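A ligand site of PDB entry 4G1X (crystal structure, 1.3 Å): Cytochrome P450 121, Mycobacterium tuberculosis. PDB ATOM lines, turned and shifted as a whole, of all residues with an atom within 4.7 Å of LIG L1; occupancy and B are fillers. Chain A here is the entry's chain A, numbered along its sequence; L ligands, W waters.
The side-chain sulfur of Met 61 sits close to an oxygen (O4) of LIG L1 (3.7 Å).
Met 85 touches LIG L1.
Ile 101 touches LIG L1.
His 145 touches LIG L1 (NE2 to C24, 3.5 Å).
Phe 229 touches LIG L1 (CZ to C31, 3.5 Å).
Gly 233 touches LIG L1.
Ser 236 touches LIG L1.
Thr 237 touches LIG L1.
Phe 240 touches LIG L1.
CZ of Phe 279 touches C2 of LIG L1 (3.6 Å).
Leu 283 touches LIG L1 (CD1 to C12, 3.7 Å).
O of Ala 336 touches C9 of LIG L1, at 3.4 Å.
Phe 337 touches LIG L1.
N of Gly 338 touches C9 of LIG L1, at 3.4 Å.
Gln 341 touches LIG L1 (O to O3, 3.8 Å).
Pro 345 touches LIG L1 (CD to C28, 3.5 Å).
Gly 346 touches LIG L1.
Hydrophobic or aromatic side chains within 4 Å of LIG L1: Met 61, Met 85, Ile 101, His 145, Phe 229, Phe 240, Phe 279, Leu 283, Phe 337, His 342 and Pro 345.
Within 4 Å of LIG L1: Met 61, Met 85, Ile 101, His 145, Phe 229, Gly 233, Ser 236, Thr 237, Phe 240, Phe 279, Leu 283, Arg 285, Ala 336, Phe 337, Gly 338, Gln 341, His 342, Cys 344, Pro 345 and Gly 346.
The nearest printed residue that does not touch LIG L1 is Leu 308 (4.04 Å).
The side-chain sulfur of Cys 344 binds an iron atom (FE1) of LIG L1 (2.2 Å).
NH2 of Arg 285 lies within salt-bridge range of O1 of LIG L1 (2.7 Å).
A ring nitrogen (ND1) of His 342 lies within hydrogen-bond range of an oxygen (O4) of LIG L1 (2.8 Å).
The side-chain hydroxyl (OG) of Ser 236 lies close to a nitrogen (N1) of LG2 L2, 3.2 Å away.
Water W5 lies within hydrogen-bond range of O4 of LIG L1 (2.6 Å) and N of Met 85 (2.9 Å).
Water W1 bridges O2 of LIG L1 (2.7 Å) and N2 of LG2 L2 (2.8 Å).
Water W3 lies within hydrogen-bond range of the backbone carbonyl oxygen (O) of Phe 343 (2.8 Å), an oxygen (O3) of LIG L1 (2.8 Å) and the backbone carbonyl oxygen (O) of Gln 341 (3.4 Å).
Water W4 lies within hydrogen-bond range of O3 of LIG L1 (2.9 Å) and O of Gln 341 (3.0 Å).
N of Cys 344 sits at hydrogen-bond distance from O of Phe 337, 2.9 Å away.
The backbone NH of Gly 346 lies close to the side-chain sulfur of Cys 344, at 3.2 Å.
A ring nitrogen (ND1) of His 342 lies within hydrogen-bond range of the side-chain sulfur (SD) of Met 61, at 3.6 Å.
The backbone carbonyl oxygen of Gly 233 lies within hydrogen-bond range of the side-chain hydroxyl of Thr 237 (2.8 Å).
A nitrogen (N1) of LG2 L2 binds an iron atom (FE1) of LIG L1, 2.4 Å away.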
ATOM      1  N   LEU A  54      25.379  -1.138  -6.400  1.00  0.00           N
ATOM      2  CA  LEU A  54      25.650  -2.125  -5.361  1.00  0.00           C
ATOM      3  C   LEU A  54      27.024  -1.915  -4.625  1.00  0.00           C
ATOM      4  O   LEU A  54      27.160  -2.372  -3.515  1.00  0.00           O
ATOM      5  CB  LEU A  54      25.666  -3.540  -5.929  1.00  0.00           C
ATOM      6  CG  LEU A  54      24.238  -4.021  -6.351  1.00  0.00           C
ATOM      7  CD1 LEU A  54      24.365  -5.369  -6.985  1.00  0.00           C
ATOM      8  CD2 LEU A  54      23.230  -4.014  -5.217  1.00  0.00           C
ATOM      9  N   MET A  61      21.089  -0.500   2.169  1.00  0.00           N
ATOM     10  CA  MET A  61      20.063  -1.497   2.439  1.00  0.00           C
ATOM     11  C   MET A  61      19.349  -1.124   3.691  1.00  0.00           C
ATOM     12  O   MET A  61      18.086  -1.158   3.729  1.00  0.00           O
ATOM     13  CB  MET A  61      20.716  -2.895   2.560  1.00  0.00           C
ATOM     14  CG  MET A  61      19.759  -3.973   3.050  1.00  0.00           C
ATOM     15  SD  MET A  61      20.482  -5.600   3.299  1.00  0.00           S
ATOM     16  CE  MET A  61      20.695  -6.095   1.658  1.00  0.00           C
ATOM     17  N   MET A  85      22.651  -8.824   8.544  1.00  0.00           N
ATOM     18  CA  MET A  85      24.065  -9.190   8.508  1.00  0.00           C
ATOM     19  C   MET A  85      24.875  -8.080   9.203  1.00  0.00           C
ATOM     20  O   MET A  85      25.900  -8.451   9.885  1.00  0.00           O
ATOM     21  CB  MET A  85      24.484  -9.435   7.032  1.00  0.00           C
ATOM     22  CG  MET A  85      25.788 -10.282   6.805  1.00  0.00           C
ATOM     23  SD  MET A  85      25.492 -11.973   7.319  1.00  0.00           S
ATOM     24  N   ILE A 101      28.016 -21.859   7.332  1.00  0.00           N
ATOM     25  CA  ILE A 101      27.113 -22.043   6.158  1.00  0.00           C
ATOM     26  C   ILE A 101      27.922 -22.258   4.903  1.00  0.00           C
ATOM     27  O   ILE A 101      27.290 -22.052   3.780  1.00  0.00           O
ATOM     28  CB  ILE A 101      26.112 -20.853   6.020  1.00  0.00           C
ATOM     29  CG1 ILE A 101      26.845 -19.540   5.704  1.00  0.00           C
ATOM     30  CG2 ILE A 101      25.270 -20.724   7.265  1.00  0.00           C
ATOM     31  CD1 ILE A 101      25.883 -18.407   5.236  1.00  0.00           C
ATOM     32  N   HIS A 145      19.099 -27.230   4.791  1.00  0.00           N
ATOM     33  CA  HIS A 145      19.156 -26.184   5.809  1.00  0.00           C
ATOM     34  C   HIS A 145      18.889 -26.730   7.145  1.00  0.00           C
ATOM     35  O   HIS A 145      19.483 -26.181   8.128  1.00  0.00           O
ATOM     36  CB  HIS A 145      18.272 -24.976   5.413  1.00  0.00           C
ATOM     37  CG  HIS A 145      18.888 -24.212   4.330  1.00  0.00           C
ATOM     38  ND1 HIS A 145      18.877 -24.592   3.005  1.00  0.00           N
ATOM     39  CD2 HIS A 145      19.691 -23.066   4.334  1.00  0.00           C
ATOM     40  CE1 HIS A 145      19.586 -23.690   2.273  1.00  0.00           C
ATOM     41  NE2 HIS A 145      20.059 -22.745   3.059  1.00  0.00           N
ATOM     42  N   PHE A 229      18.311 -17.182   8.406  1.00  0.00           N
ATOM     43  CA  PHE A 229      19.174 -17.978   7.568  1.00  0.00           C
ATOM     44  C   PHE A 229      18.418 -19.224   7.078  1.00  0.00           C
ATOM     45  O   PHE A 229      18.582 -19.574   5.858  1.00  0.00           O
ATOM     46  CB  PHE A 229      20.537 -18.352   8.273  1.00  0.00           C
ATOM     47  CG  PHE A 229      21.530 -17.253   8.185  1.00  0.00           C
ATOM     48  CD1 PHE A 229      21.257 -15.954   8.668  1.00  0.00           C
ATOM     49  CD2 PHE A 229      22.737 -17.460   7.585  1.00  0.00           C
ATOM     50  CE1 PHE A 229      22.200 -14.955   8.546  1.00  0.00           C
ATOM     51  CE2 PHE A 229      23.690 -16.442   7.471  1.00  0.00           C
ATOM     52  CZ  PHE A 229      23.402 -15.192   7.960  1.00  0.00           C
ATOM     53  N   GLY A 233      17.806 -18.937   3.055  1.00  0.00           N
ATOM     54  CA  GLY A 233      18.599 -19.938   2.388  1.00  0.00           C
ATOM     55  C   GLY A 233      17.670 -20.935   1.666  1.00  0.00           C
ATOM     56  O   GLY A 233      17.942 -21.306   0.507  1.00  0.00           O
ATOM     57  N   SER A 236      15.900 -19.253  -1.317  1.00  0.00           N
ATOM     58  CA  SER A 236      16.771 -18.864  -2.387  1.00  0.00           C
ATOM     59  C   SER A 236      17.315 -20.073  -3.146  1.00  0.00           C
ATOM     60  O   SER A 236      17.297 -20.126  -4.379  1.00  0.00           O
ATOM     61  CB  SER A 236      17.975 -18.055  -1.869  1.00  0.00           C
ATOM     62  OG  SER A 236      17.542 -16.840  -1.262  1.00  0.00           O
ATOM     63  N   THR A 237      17.714 -21.118  -2.413  1.00  0.00           N
ATOM     64  CA  THR A 237      18.234 -22.322  -3.033  1.00  0.00           C
ATOM     65  C   THR A 237      17.114 -23.127  -3.677  1.00  0.00           C
ATOM     66  O   THR A 237      17.299 -23.637  -4.823  1.00  0.00           O
ATOM     67  CB  THR A 237      19.014 -23.262  -2.044  1.00  0.00           C
ATOM     68  OG1 THR A 237      18.211 -23.625  -0.952  1.00  0.00           O
ATOM     69  CG2 THR A 237      20.331 -22.574  -1.585  1.00  0.00           C
ATOM     70  N   PHE A 240      16.004 -21.118  -6.835  1.00  0.00           N
ATOM     71  CA  PHE A 240      17.018 -21.141  -7.890  1.00  0.00           C
ATOM     72  C   PHE A 240      17.088 -22.549  -8.509  1.00  0.00           C
ATOM     73  O   PHE A 240      17.059 -22.628  -9.758  1.00  0.00           O
ATOM     74  CB  PHE A 240      18.402 -20.757  -7.331  1.00  0.00           C
ATOM     75  CG  PHE A 240      19.457 -21.019  -8.360  1.00  0.00           C
ATOM     76  CD1 PHE A 240      19.417 -20.388  -9.609  1.00  0.00           C
ATOM     77  CD2 PHE A 240      20.457 -22.022  -8.137  1.00  0.00           C
ATOM     78  CE1 PHE A 240      20.321 -20.763 -10.640  1.00  0.00           C
ATOM     79  CE2 PHE A 240      21.333 -22.341  -9.164  1.00  0.00           C
ATOM     80  CZ  PHE A 240      21.263 -21.761 -10.374  1.00  0.00           C
ATOM     81  N   LEU A 273      23.045 -19.836 -12.914  1.00  0.00           N
ATOM     82  CA  LEU A 273      22.964 -18.647 -12.011  1.00  0.00           C
ATOM     83  C   LEU A 273      22.920 -17.434 -12.790  1.00  0.00           C
ATOM     84  O   LEU A 273      22.066 -16.528 -12.535  1.00  0.00           O
ATOM     85  CB  LEU A 273      24.161 -18.619 -11.075  1.00  0.00           C
ATOM     86  CG  LEU A 273      24.078 -19.634  -9.947  1.00  0.00           C
ATOM     87  CD1 LEU A 273      25.464 -19.889  -9.296  1.00  0.00           C
ATOM     88  CD2 LEU A 273      23.107 -19.110  -8.830  1.00  0.00           C
ATOM     89  N   PHE A 279      14.858 -13.921  -8.790  1.00  0.00           N
ATOM     90  CA  PHE A 279      14.479 -12.709  -8.063  1.00  0.00           C
ATOM     91  C   PHE A 279      13.411 -11.930  -8.763  1.00  0.00           C
ATOM     92  O   PHE A 279      13.567 -11.547  -9.884  1.00  0.00           O
ATOM     93  CB  PHE A 279      15.721 -11.817  -7.804  1.00  0.00           C
ATOM     94  CG  PHE A 279      16.538 -12.314  -6.661  1.00  0.00           C
ATOM     95  CD1 PHE A 279      17.213 -13.520  -6.737  1.00  0.00           C
ATOM     96  CD2 PHE A 279      16.535 -11.617  -5.437  1.00  0.00           C
ATOM     97  CE1 PHE A 279      17.954 -13.968  -5.610  1.00  0.00           C
ATOM     98  CE2 PHE A 279      17.262 -12.160  -4.333  1.00  0.00           C
ATOM     99  CZ  PHE A 279      17.900 -13.343  -4.470  1.00  0.00           C
ATOM    100  N   LEU A 283      16.828  -5.473  -6.424  1.00  0.00           N
ATOM    101  CA  LEU A 283      17.282  -5.361  -5.050  1.00  0.00           C
ATOM    102  C   LEU A 283      17.136  -3.878  -4.617  1.00  0.00           C
ATOM    103  O   LEU A 283      17.610  -2.982  -5.318  1.00  0.00           O
ATOM    104  CB  LEU A 283      18.804  -5.711  -4.946  1.00  0.00           C
ATOM    105  CG  LEU A 283      19.168  -7.126  -5.484  1.00  0.00           C
ATOM    106  CD1 LEU A 283      20.671  -7.296  -5.282  1.00  0.00           C
ATOM    107  CD2 LEU A 283      18.368  -8.181  -4.755  1.00  0.00           C
ATOM    108  N   ARG A 285      17.529  -0.312  -2.528  1.00  0.00           N
ATOM    109  CA  ARG A 285      18.413   0.505  -1.747  1.00  0.00           C
ATOM    110  C   ARG A 285      17.809   1.908  -1.577  1.00  0.00           C
ATOM    111  O   ARG A 285      17.103   2.334  -2.509  1.00  0.00           O
ATOM    112  CB  ARG A 285      19.759   0.668  -2.544  1.00  0.00           C
ATOM    113  CG  ARG A 285      20.601  -0.611  -2.723  1.00  0.00           C
ATOM    114  CD  ARG A 285      21.121  -1.097  -1.421  1.00  0.00           C
ATOM    115  NE  ARG A 285      22.077  -2.205  -1.608  1.00  0.00           N
ATOM    116  CZ  ARG A 285      21.767  -3.480  -1.643  1.00  0.00           C
ATOM    117  NH1 ARG A 285      20.537  -3.945  -1.509  1.00  0.00           N
ATOM    118  NH2 ARG A 285      22.758  -4.395  -1.734  1.00  0.00           N
ATOM    119  N   LEU A 308      18.575  -7.496 -11.298  1.00  0.00           N
ATOM    120  CA  LEU A 308      19.718  -8.475 -11.521  1.00  0.00           C
ATOM    121  C   LEU A 308      19.671  -8.977 -12.907  1.00  0.00           C
ATOM    122  O   LEU A 308      20.790  -9.097 -13.523  1.00  0.00           O
ATOM    123  CB  LEU A 308      19.597  -9.577 -10.482  1.00  0.00           C
ATOM    124  CG  LEU A 308      19.771  -9.169  -9.047  1.00  0.00           C
ATOM    125  CD1 LEU A 308      19.747 -10.394  -8.140  1.00  0.00           C
ATOM    126  CD2 LEU A 308      21.036  -8.304  -8.814  1.00  0.00           C
ATOM    127  N   LEU A 335      25.764 -11.074 -11.296  1.00  0.00           N
ATOM    128  CA  LEU A 335      25.254 -10.471 -10.050  1.00  0.00           C
ATOM    129  C   LEU A 335      24.250 -11.373  -9.422  1.00  0.00           C
ATOM    130  O   LEU A 335      23.471 -10.862  -8.562  1.00  0.00           O
ATOM    131  CB  LEU A 335      24.721  -9.082 -10.286  1.00  0.00           C
ATOM    132  CG  LEU A 335      25.645  -8.110 -10.987  1.00  0.00           C
ATOM    133  CD1 LEU A 335      25.017  -6.688 -10.920  1.00  0.00           C
ATOM    134  CD2 LEU A 335      27.054  -8.090 -10.454  1.00  0.00           C
ATOM    135  N   ALA A 336      24.200 -12.675  -9.685  1.00  0.00           N
ATOM    136  CA  ALA A 336      23.142 -13.508  -9.056  1.00  0.00           C
ATOM    137  C   ALA A 336      23.239 -13.534  -7.580  1.00  0.00           C
ATOM    138  O   ALA A 336      22.221 -13.790  -6.910  1.00  0.00           O
ATOM    139  CB  ALA A 336      23.205 -14.933  -9.591  1.00  0.00           C
ATOM    140  N   PHE A 337      24.420 -13.344  -6.951  1.00  0.00           N
ATOM    141  CA  PHE A 337      24.619 -13.334  -5.499  1.00  0.00           C
ATOM    142  C   PHE A 337      24.832 -11.908  -4.990  1.00  0.00           C
ATOM    143  O   PHE A 337      25.316 -11.708  -3.877  1.00  0.00           O
ATOM    144  CB  PHE A 337      25.831 -14.191  -5.145  1.00  0.00           C
ATOM    145  CG  PHE A 337      25.600 -15.645  -5.421  1.00  0.00           C
ATOM    146  CD1 PHE A 337      24.599 -16.353  -4.714  1.00  0.00           C
ATOM    147  CD2 PHE A 337      26.463 -16.378  -6.259  1.00  0.00           C
ATOM    148  CE1 PHE A 337      24.432 -17.740  -4.933  1.00  0.00           C
ATOM    149  CE2 PHE A 337      26.275 -17.732  -6.444  1.00  0.00           C
ATOM    150  CZ  PHE A 337      25.272 -18.435  -5.795  1.00  0.00           C
ATOM    151  N   GLY A 338      24.449 -10.955  -5.800  1.00  0.00           N
ATOM    152  CA  GLY A 338      24.714  -9.554  -5.464  1.00  0.00           C
ATOM    153  C   GLY A 338      26.180  -9.135  -5.693  1.00  0.00           C
ATOM    154  O   GLY A 338      26.906  -9.797  -6.502  1.00  0.00           O
ATOM    155  N   GLN A 341      29.045  -4.835  -0.385  1.00  0.00           N
ATOM    156  CA  GLN A 341      28.886  -5.051   1.041  1.00  0.00           C
ATOM    157  C   GLN A 341      27.934  -6.201   1.348  1.00  0.00           C
ATOM    158  O   GLN A 341      28.152  -6.910   2.346  1.00  0.00           O
ATOM    159  CB  GLN A 341      28.277  -3.736   1.665  1.00  0.00           C
ATOM    160  CG  GLN A 341      27.925  -3.808   3.170  1.00  0.00           C
ATOM    161  CD  GLN A 341      29.150  -3.831   4.031  1.00  0.00           C
ATOM    162  OE1 GLN A 341      29.065  -4.058   5.252  1.00  0.00           O
ATOM    163  NE2 GLN A 341      30.254  -3.509   3.520  1.00  0.00           N
ATOM    164  N   HIS A 342      26.863  -6.367   0.553  1.00  0.00           N
ATOM    165  CA  HIS A 342      25.866  -7.376   0.905  1.00  0.00           C
ATOM    166  C   HIS A 342      25.923  -8.614   0.092  1.00  0.00           C
ATOM    167  O   HIS A 342      24.991  -9.393   0.038  1.00  0.00           O
ATOM    168  CB  HIS A 342      24.476  -6.695   0.801  1.00  0.00           C
ATOM    169  CG  HIS A 342      24.326  -5.578   1.775  1.00  0.00           C
ATOM    170  ND1 HIS A 342      24.099  -5.817   3.094  1.00  0.00           N
ATOM    171  CD2 HIS A 342      24.365  -4.236   1.602  1.00  0.00           C
ATOM    172  CE1 HIS A 342      24.042  -4.610   3.758  1.00  0.00           C
ATOM    173  NE2 HIS A 342      24.224  -3.661   2.868  1.00  0.00           N
ATOM    174  N   PHE A 343      27.101  -8.872  -0.589  1.00  0.00           N
ATOM    175  CA  PHE A 343      27.256 -10.074  -1.399  1.00  0.00           C
ATOM    176  C   PHE A 343      26.906 -11.331  -0.571  1.00  0.00           C
ATOM    177  O   PHE A 343      27.236 -11.464   0.647  1.00  0.00           O
ATOM    178  CB  PHE A 343      28.763 -10.216  -1.709  1.00  0.00           C
ATOM    179  CG  PHE A 343      29.061 -11.423  -2.602  1.00  0.00           C
ATOM    180  CD1 PHE A 343      28.792 -11.388  -3.919  1.00  0.00           C
ATOM    181  CD2 PHE A 343      29.554 -12.557  -2.015  1.00  0.00           C
ATOM    182  CE1 PHE A 343      29.041 -12.509  -4.775  1.00  0.00           C
ATOM    183  CE2 PHE A 343      29.770 -13.727  -2.817  1.00  0.00           C
ATOM    184  CZ  PHE A 343      29.506 -13.663  -4.134  1.00  0.00           C
ATOM    185  N   CYS A 344      26.154 -12.245  -1.153  1.00  0.00           N
ATOM    186  CA  CYS A 344      25.541 -13.397  -0.432  1.00  0.00           C
ATOM    187  C   CYS A 344      26.600 -14.263   0.346  1.00  0.00           C
ATOM    188  O   CYS A 344      27.489 -14.816  -0.381  1.00  0.00           O
ATOM    189  CB  CYS A 344      24.858 -14.297  -1.468  1.00  0.00           C
ATOM    190  SG  CYS A 344      23.998 -15.661  -0.661  1.00  0.00           S
ATOM    191  N   PRO A 345      26.477 -14.408   1.592  1.00  0.00           N
ATOM    192  CA  PRO A 345      27.460 -15.302   2.297  1.00  0.00           C
ATOM    193  C   PRO A 345      27.115 -16.724   2.073  1.00  0.00           C
ATOM    194  O   PRO A 345      27.885 -17.638   2.448  1.00  0.00           O
ATOM    195  CB  PRO A 345      27.290 -14.885   3.787  1.00  0.00           C
ATOM    196  CG  PRO A 345      25.806 -14.476   3.837  1.00  0.00           C
ATOM    197  CD  PRO A 345      25.563 -13.710   2.516  1.00  0.00           C
ATOM    198  N   GLY A 346      25.941 -17.058   1.509  1.00  0.00           N
ATOM    199  CA  GLY A 346      25.558 -18.462   1.202  1.00  0.00           C
ATOM    200  C   GLY A 346      25.994 -18.861  -0.244  1.00  0.00           C
ATOM    201  O   GLY A 346      25.533 -19.939  -0.652  1.00  0.00           O
ATOM    202  N   LEU A 349      27.449 -22.440  -0.677  1.00  0.00           N
ATOM    203  CA  LEU A 349      26.450 -23.415  -0.341  1.00  0.00           C
ATOM    204  C   LEU A 349      25.330 -23.522  -1.439  1.00  0.00           C
ATOM    205  O   LEU A 349      24.866 -24.634  -1.776  1.00  0.00           O
ATOM    206  CB  LEU A 349      25.787 -23.162   1.009  1.00  0.00           C
ATOM    207  CG  LEU A 349      24.832 -24.151   1.600  1.00  0.00           C
ATOM    208  CD1 LEU A 349      25.578 -25.501   1.838  1.00  0.00           C
ATOM    209  CD2 LEU A 349      24.247 -23.656   2.895  1.00  0.00           C
ATOM    210  N   GLY A 350      24.926 -22.352  -1.938  1.00  0.00           N
ATOM    211  CA  GLY A 350      23.927 -22.367  -2.966  1.00  0.00           C
ATOM    212  C   GLY A 350      24.418 -22.996  -4.264  1.00  0.00           C
ATOM    213  O   GLY A 350      23.703 -23.807  -4.891  1.00  0.00           O
HETATM  214  C1  LIG L   1      22.286 -11.892   0.334  1.00  0.00           C
HETATM  215  C2  LIG L   1      21.184 -14.475  -3.696  1.00  0.00           C
HETATM  216  C3  LIG L   1      21.571 -18.588  -1.138  1.00  0.00           C
HETATM  217  C4  LIG L   1      21.946 -15.913   2.911  1.00  0.00           C
HETATM  218  C5  LIG L   1      22.049 -12.296  -1.016  1.00  0.00           C
HETATM  219  C6  LIG L   1      21.979 -11.330  -2.118  1.00  0.00           C
HETATM  220  C7  LIG L   1      21.583 -12.031  -3.258  1.00  0.00           C
HETATM  221  C8  LIG L   1      21.485 -13.418  -2.865  1.00  0.00           C
HETATM  222  C9  LIG L   1      21.301 -11.461  -4.562  1.00  0.00           C
HETATM  223  C10 LIG L   1      22.255  -9.832  -2.043  1.00  0.00           C
HETATM  224  C11 LIG L   1      21.037  -8.993  -1.608  1.00  0.00           C
HETATM  225  C12 LIG L   1      21.290  -7.530  -1.685  1.00  0.00           C
HETATM  226  O1  LIG L   1      22.423  -7.066  -1.880  1.00  0.00           O
HETATM  227  O2  LIG L   1      20.247  -6.731  -1.587  1.00  0.00           O
HETATM  228  C13 LIG L   1      21.180 -15.815  -3.306  1.00  0.00           C
HETATM  229  C14 LIG L   1      21.018 -16.844  -4.221  1.00  0.00           C
HETATM  230  C15 LIG L   1      21.117 -18.050  -3.507  1.00  0.00           C
HETATM  231  C16 LIG L   1      21.365 -17.604  -2.156  1.00  0.00           C
HETATM  232  C17 LIG L   1      20.741 -16.718  -5.653  1.00  0.00           C
HETATM  233  C18 LIG L   1      21.000 -19.451  -3.948  1.00  0.00           C
HETATM  234  C19 LIG L   1      21.289 -19.965  -5.126  1.00  0.00           C
HETATM  235  C20 LIG L   1      21.815 -18.161   0.162  1.00  0.00           C
HETATM  236  C21 LIG L   1      21.978 -19.150   1.240  1.00  0.00           C
HETATM  237  C22 LIG L   1      21.974 -18.396   2.442  1.00  0.00           C
HETATM  238  C23 LIG L   1      21.921 -17.010   2.075  1.00  0.00           C
HETATM  239  C24 LIG L   1      22.151 -20.631   1.200  1.00  0.00           C
HETATM  240  C25 LIG L   1      22.161 -18.906   3.864  1.00  0.00           C
HETATM  241  C26 LIG L   1      22.046 -20.118   4.426  1.00  0.00           C
HETATM  242  C27 LIG L   1      22.077 -14.561   2.564  1.00  0.00           C
HETATM  243  C28 LIG L   1      22.235 -13.503   3.564  1.00  0.00           C
HETATM  244  C29 LIG L   1      22.330 -12.365   2.814  1.00  0.00           C
HETATM  245  C30 LIG L   1      22.207 -12.778   1.420  1.00  0.00           C
HETATM  246  C31 LIG L   1      22.284 -13.657   5.056  1.00  0.00           C
HETATM  247  C32 LIG L   1      22.460 -10.927   3.314  1.00  0.00           C
HETATM  248  C33 LIG L   1      23.868 -10.426   3.292  1.00  0.00           C
HETATM  249  C34 LIG L   1      23.965  -8.958   3.710  1.00  0.00           C
HETATM  250  O3  LIG L   1      25.169  -8.685   3.814  1.00  0.00           O
HETATM  251  O4  LIG L   1      23.000  -8.213   3.881  1.00  0.00           O
HETATM  252  N1  LIG L   1      21.720 -13.608  -1.473  1.00  0.00           N
HETATM  253  N2  LIG L   1      21.331 -16.256  -2.052  1.00  0.00           N
HETATM  254  N3  LIG L   1      21.743 -16.889   0.654  1.00  0.00           N
HETATM  255  N4  LIG L   1      22.107 -14.103   1.301  1.00  0.00           N
HETATM  256 FE1  LIG L   1      21.864 -15.211  -0.398  1.00  0.00          FE
HETATM  257  C1  LG2 L   2      18.714 -11.791   1.839  1.00  0.00           C
HETATM  258  C2  LG2 L   2      19.125 -13.114   1.748  1.00  0.00           C
HETATM  259  C3  LG2 L   2      19.214 -13.719   0.498  1.00  0.00           C
HETATM  260  N1  LG2 L   2      19.593 -14.992   0.404  1.00  0.00           N
HETATM  261  C4  LG2 L   2      18.903 -13.000  -0.652  1.00  0.00           C
HETATM  262  C5  LG2 L   2      18.504 -11.676  -0.553  1.00  0.00           C
HETATM  263  C6  LG2 L   2      18.407 -11.066   0.696  1.00  0.00           C
HETATM  264  N2  LG2 L   2      18.022  -9.782   0.783  1.00  0.00           N
HETATM  265  C7  LG2 L   2      17.921  -9.174   1.953  1.00  0.00           C
HETATM  266  C8  LG2 L   2      18.218  -9.847   3.138  1.00  0.00           C
HETATM  267  C9  LG2 L   2      18.621 -11.176   3.082  1.00  0.00           C
HETATM  268  N3  LG2 L   2      18.908 -11.840   4.194  1.00  0.00           N
HETATM  269  C10 LG2 L   2      19.560 -11.398   5.262  1.00  0.00           C
HETATM  270  N4  LG2 L   2      19.624 -12.403   6.129  1.00  0.00           N
HETATM  271  C11 LG2 L   2      18.997 -13.423   5.554  1.00  0.00           C
HETATM  272  N5  LG2 L   2      18.575 -13.010   4.348  1.00  0.00           N
HETATM  273  O   HOH W   1      17.715  -7.603  -0.992  1.00  0.00           O
HETATM  274  O   HOH W   2      24.775  -7.329  -2.915  1.00  0.00           O
HETATM  275  O   HOH W   3      27.492 -10.152   3.116  1.00  0.00           O
HETATM  276  O   HOH W   4      27.092  -7.033   5.188  1.00  0.00           O
HETATM  277  O   HOH W   5      21.361  -8.298   5.955  1.00  0.00           O
